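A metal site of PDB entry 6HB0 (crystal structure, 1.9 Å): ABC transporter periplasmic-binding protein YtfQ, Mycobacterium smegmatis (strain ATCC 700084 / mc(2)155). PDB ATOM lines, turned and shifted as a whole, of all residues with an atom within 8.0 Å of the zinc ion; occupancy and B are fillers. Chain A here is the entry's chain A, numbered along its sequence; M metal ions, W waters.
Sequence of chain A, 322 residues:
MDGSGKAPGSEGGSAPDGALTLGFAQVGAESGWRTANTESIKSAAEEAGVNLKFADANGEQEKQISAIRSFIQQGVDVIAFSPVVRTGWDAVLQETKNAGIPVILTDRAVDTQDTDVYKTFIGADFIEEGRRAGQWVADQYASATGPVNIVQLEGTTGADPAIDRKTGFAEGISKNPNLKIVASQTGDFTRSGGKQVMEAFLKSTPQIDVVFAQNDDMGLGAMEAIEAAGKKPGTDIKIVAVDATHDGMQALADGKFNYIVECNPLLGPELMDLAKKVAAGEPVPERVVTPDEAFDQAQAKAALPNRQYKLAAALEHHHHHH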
ATOM      1  N   GLY A 123      22.031   6.400   7.395  1.00  0.00           N
ATOM      2  CA  GLY A 123      20.683   6.866   7.785  1.00  0.00           C
ATOM      3  C   GLY A 123      19.926   5.881   8.649  1.00  0.00           C
ATOM      4  O   GLY A 123      20.383   4.778   8.817  1.00  0.00           O
ATOM      5  N   ALA A 124      18.778   6.309   9.162  1.00  0.00           N
ATOM      6  CA  ALA A 124      17.995   5.496  10.072  1.00  0.00           C
ATOM      7  C   ALA A 124      17.288   4.391   9.311  1.00  0.00           C
ATOM      8  O   ALA A 124      17.048   4.526   8.112  1.00  0.00           O
ATOM      9  CB  ALA A 124      16.974   6.325  10.814  1.00  0.00           C
ATOM     10  N   ASP A 125      17.001   3.305  10.016  1.00  0.00           N
ATOM     11  CA  ASP A 125      16.266   2.174   9.509  1.00  0.00           C
ATOM     12  C   ASP A 125      14.852   2.053  10.118  1.00  0.00           C
ATOM     13  O   ASP A 125      14.662   1.549  11.248  1.00  0.00           O
ATOM     14  CB  ASP A 125      17.051   0.935   9.874  1.00  0.00           C
ATOM     15  CG  ASP A 125      16.563  -0.336   9.160  1.00  0.00           C
ATOM     16  OD1 ASP A 125      15.419  -0.381   8.644  1.00  0.00           O
ATOM     17  OD2 ASP A 125      17.335  -1.305   9.153  1.00  0.00           O
ATOM     18  N   PHE A 126      13.837   2.475   9.372  1.00  0.00           N
ATOM     19  CA  PHE A 126      12.491   2.487   9.919  1.00  0.00           C
ATOM     20  C   PHE A 126      11.866   1.099  10.050  1.00  0.00           C
ATOM     21  O   PHE A 126      11.023   0.879  10.929  1.00  0.00           O
ATOM     22  CB  PHE A 126      11.595   3.333   9.042  1.00  0.00           C
ATOM     23  CG  PHE A 126      12.058   4.748   8.882  1.00  0.00           C
ATOM     24  CD1 PHE A 126      12.415   5.512   9.995  1.00  0.00           C
ATOM     25  CD2 PHE A 126      12.152   5.316   7.623  1.00  0.00           C
ATOM     26  CE1 PHE A 126      12.819   6.814   9.853  1.00  0.00           C
ATOM     27  CE2 PHE A 126      12.592   6.616   7.471  1.00  0.00           C
ATOM     28  CZ  PHE A 126      12.893   7.361   8.587  1.00  0.00           C
ATOM     29  N   GLU A 128      13.553  -1.549  10.891  1.00  0.00           N
ATOM     30  CA  GLU A 128      14.154  -1.986  12.144  1.00  0.00           C
ATOM     31  C   GLU A 128      13.410  -1.425  13.350  1.00  0.00           C
ATOM     32  O   GLU A 128      13.200  -2.140  14.322  1.00  0.00           O
ATOM     33  CB  GLU A 128      15.630  -1.615  12.145  1.00  0.00           C
ATOM     34  CG  GLU A 128      16.380  -1.842  13.430  1.00  0.00           C
ATOM     35  CD  GLU A 128      16.986  -0.534  13.925  1.00  0.00           C
ATOM     36  OE1 GLU A 128      16.357   0.136  14.782  1.00  0.00           O
ATOM     37  OE2 GLU A 128      18.055  -0.137  13.374  1.00  0.00           O
ATOM     38  N   GLU A 129      13.000  -0.164  13.331  1.00  0.00           N
ATOM     39  CA  GLU A 129      12.185   0.401  14.411  1.00  0.00           C
ATOM     40  C   GLU A 129      10.916  -0.393  14.677  1.00  0.00           C
ATOM     41  O   GLU A 129      10.626  -0.751  15.808  1.00  0.00           O
ATOM     42  CB  GLU A 129      11.797   1.882  14.174  1.00  0.00           C
ATOM     43  CG  GLU A 129      12.999   2.851  14.286  1.00  0.00           C
ATOM     44  CD  GLU A 129      12.616   4.305  13.981  1.00  0.00           C
ATOM     45  OE1 GLU A 129      11.796   4.519  13.033  1.00  0.00           O
ATOM     46  OE2 GLU A 129      13.160   5.223  14.691  1.00  0.00           O
ATOM     47  N   ARG A 132      11.693  -3.867  16.068  1.00  0.00           N
ATOM     48  CA  ARG A 132      12.047  -3.903  17.514  1.00  0.00           C
ATOM     49  C   ARG A 132      10.792  -3.700  18.368  1.00  0.00           C
ATOM     50  O   ARG A 132      10.666  -4.284  19.463  1.00  0.00           O
ATOM     51  CB  ARG A 132      13.163  -2.876  17.817  1.00  0.00           C
ATOM     52  CG  ARG A 132      14.481  -3.222  17.116  1.00  0.00           C
ATOM     53  CD  ARG A 132      15.399  -2.029  16.904  1.00  0.00           C
ATOM     54  NE  ARG A 132      15.592  -1.403  18.167  1.00  0.00           N
ATOM     55  CZ  ARG A 132      15.753  -0.100  18.385  1.00  0.00           C
ATOM     56  NH1 ARG A 132      15.880   0.824  17.431  1.00  0.00           N
ATOM     57  NH2 ARG A 132      15.826   0.270  19.653  1.00  0.00           N
ATOM     58  N   GLU A 262      13.788   3.783  19.108  1.00  0.00           N
ATOM     59  CA  GLU A 262      14.162   4.779  18.098  1.00  0.00           C
ATOM     60  C   GLU A 262      15.386   4.314  17.417  1.00  0.00           C
ATOM     61  O   GLU A 262      16.265   3.764  18.065  1.00  0.00           O
ATOM     62  CB  GLU A 262      14.417   6.137  18.720  1.00  0.00           C
ATOM     63  CG  GLU A 262      14.726   7.198  17.676  1.00  0.00           C
ATOM     64  CD  GLU A 262      15.004   8.576  18.235  1.00  0.00           C
ATOM     65  OE1 GLU A 262      14.239   8.990  19.114  1.00  0.00           O
ATOM     66  OE2 GLU A 262      15.960   9.268  17.750  1.00  0.00           O
ATOM     67  N   CYS A 263      15.450   4.486  16.097  1.00  0.00           N
ATOM     68  CA  CYS A 263      16.653   4.349  15.337  1.00  0.00           C
ATOM     69  C   CYS A 263      17.105   5.794  15.095  1.00  0.00           C
ATOM     70  O   CYS A 263      16.374   6.587  14.485  1.00  0.00           O
ATOM     71  CB  CYS A 263      16.433   3.659  14.005  1.00  0.00           C
ATOM     72  SG  CYS A 263      17.960   3.375  13.078  1.00  0.00           S
ATOM     73  N   ASN A 264      18.285   6.146  15.553  1.00  0.00           N
ATOM     74  CA  ASN A 264      18.762   7.514  15.413  1.00  0.00           C
ATOM     75  C   ASN A 264      19.070   7.912  13.952  1.00  0.00           C
ATOM     76  O   ASN A 264      19.415   7.108  13.110  1.00  0.00           O
ATOM     77  CB  ASN A 264      20.073   7.735  16.178  1.00  0.00           C
ATOM     78  CG  ASN A 264      19.933   7.735  17.662  1.00  0.00           C
ATOM     79  OD1 ASN A 264      20.919   7.502  18.338  1.00  0.00           O
ATOM     80  ND2 ASN A 264      18.777   8.031  18.190  1.00  0.00           N
ATOM     81  N   PRO A 265      18.950   9.211  13.685  1.00  0.00           N
ATOM     82  CA  PRO A 265      19.633   9.695  12.493  1.00  0.00           C
ATOM     83  C   PRO A 265      21.147   9.689  12.686  1.00  0.00           C
ATOM     84  O   PRO A 265      21.688   9.363  13.782  1.00  0.00           O
ATOM     85  CB  PRO A 265      19.135  11.128  12.366  1.00  0.00           C
ATOM     86  CG  PRO A 265      18.947  11.541  13.784  1.00  0.00           C
ATOM     87  CD  PRO A 265      18.455  10.297  14.516  1.00  0.00           C
ATOM     88  N   ARG A 287      27.077   0.993   3.416  1.00  0.00           N
ATOM     89  CA  ARG A 287      26.131   1.458   4.409  1.00  0.00           C
ATOM     90  C   ARG A 287      26.805   1.491   5.781  1.00  0.00           C
ATOM     91  O   ARG A 287      27.595   0.598   6.097  1.00  0.00           O
ATOM     92  CB  ARG A 287      24.927   0.514   4.440  1.00  0.00           C
ATOM     93  CG  ARG A 287      23.863   0.983   5.391  1.00  0.00           C
ATOM     94  CD  ARG A 287      22.537   0.292   5.205  1.00  0.00           C
ATOM     95  NE  ARG A 287      21.789   0.506   6.460  1.00  0.00           N
ATOM     96  CZ  ARG A 287      21.158  -0.423   7.187  1.00  0.00           C
ATOM     97  NH1 ARG A 287      21.071  -1.684   6.752  1.00  0.00           N
ATOM     98  NH2 ARG A 287      20.544  -0.079   8.337  1.00  0.00           N
ATOM     99  N   VAL A 289      25.606   2.038   9.823  1.00  0.00           N
ATOM    100  CA  VAL A 289      24.406   2.062  10.627  1.00  0.00           C
ATOM    101  C   VAL A 289      24.417   3.128  11.670  1.00  0.00           C
ATOM    102  O   VAL A 289      25.453   3.514  12.130  1.00  0.00           O
ATOM    103  CB  VAL A 289      24.203   0.750  11.448  1.00  0.00           C
ATOM    104  CG1 VAL A 289      24.027  -0.385  10.484  1.00  0.00           C
ATOM    105  CG2 VAL A 289      25.355   0.503  12.441  1.00  0.00           C
ATOM    106  N   THR A 290      23.254   3.643  11.995  1.00  0.00           N
ATOM    107  CA  THR A 290      23.163   4.643  13.033  1.00  0.00           C
ATOM    108  C   THR A 290      22.939   3.910  14.358  1.00  0.00           C
ATOM    109  O   THR A 290      22.491   2.789  14.366  1.00  0.00           O
ATOM    110  CB  THR A 290      22.024   5.624  12.768  1.00  0.00           C
ATOM    111  OG1 THR A 290      20.800   4.897  12.578  1.00  0.00           O
ATOM    112  CG2 THR A 290      22.315   6.458  11.537  1.00  0.00           C
ATOM    113  N   PRO A 291      23.217   4.580  15.474  1.00  0.00           N
ATOM    114  CA  PRO A 291      22.852   3.997  16.752  1.00  0.00           C
ATOM    115  C   PRO A 291      21.346   3.949  17.058  1.00  0.00           C
ATOM    116  O   PRO A 291      20.554   4.677  16.463  1.00  0.00           O
ATOM    117  CB  PRO A 291      23.546   4.925  17.777  1.00  0.00           C
ATOM    118  CG  PRO A 291      24.162   6.012  17.029  1.00  0.00           C
ATOM    119  CD  PRO A 291      23.786   5.924  15.602  1.00  0.00           C
ATOM    120  N   ASP A 292      20.999   3.129  18.042  1.00  0.00           N
ATOM    121  CA  ASP A 292      19.662   2.947  18.502  1.00  0.00           C
ATOM    122  C   ASP A 292      19.453   3.355  19.925  1.00  0.00           C
ATOM    123  O   ASP A 292      20.394   3.414  20.717  1.00  0.00           O
ATOM    124  CB  ASP A 292      19.314   1.452  18.364  1.00  0.00           C
ATOM    125  CG  ASP A 292      19.229   0.995  16.918  1.00  0.00           C
ATOM    126  OD1 ASP A 292      18.910   1.826  16.037  1.00  0.00           O
ATOM    127  OD2 ASP A 292      19.455  -0.211  16.663  1.00  0.00           O
ATOM    128  N   GLU A 293      18.188   3.628  20.272  1.00  0.00           N
ATOM    129  CA  GLU A 293      17.752   3.866  21.628  1.00  0.00           C
ATOM    130  C   GLU A 293      16.558   2.978  21.901  1.00  0.00           C
ATOM    131  O   GLU A 293      15.768   2.638  20.975  1.00  0.00           O
ATOM    132  CB  GLU A 293      17.337   5.310  21.859  1.00  0.00           C
ATOM    133  CG  GLU A 293      18.474   6.289  21.620  1.00  0.00           C
ATOM    134  CD  GLU A 293      18.089   7.767  21.805  1.00  0.00           C
ATOM    135  OE1 GLU A 293      17.463   8.094  22.817  1.00  0.00           O
ATOM    136  OE2 GLU A 293      18.511   8.596  20.982  1.00  0.00           O
HETATM  137 ZN    ZN M   1      18.772   1.541  14.144  1.00  0.00          ZN
HETATM  138  O   HOH W   1      20.643   1.193  13.454  1.00  0.00           O
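Thr 290 touches the zinc ion. Along chain A the residues within 4 Å of the zinc ion span positions 128 to 292. The nearest printed residue that does not touch the zinc ion is Pro 291 (4.3 Å).
OD2 of Asp 292 is in salt-bridge range of NH1 of Arg 132 (3.8 Å). The side-chain carboxylate (OE1) of Glu 128 lies within salt-bridge range of the guanidinium group (NH1) of Arg 132 (2.8 Å). The side-chain carboxylate of Asp 125 lies within hydrogen-bond range of the backbone NH of Glu 128 (3.1 Å). The side-chain sulfur (SG) of Cys 263 sits close to the side-chain hydroxyl (OG1) of Thr 290 (3.3 Å). The backbone NH of Asp 125 lies close to the side-chain sulfur of Cys 263, 3.2 Å away. The backbone NH of Cys 263 lies within hydrogen-bond range of the side-chain carboxylate of Glu 129, at 2.8 Å. The backbone carbonyl oxygen (O) of Asn 264 sits at hydrogen-bond distance from the side-chain hydroxyl (OG1) of Thr 290 (2.7 Å).
The zinc ion is bound by the side-chain carboxylate (OD1) of Asp 292, the side-chain carboxylate (OE2) of Glu 128, water W1 and the side-chain sulfur (SG) of Cys 263.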
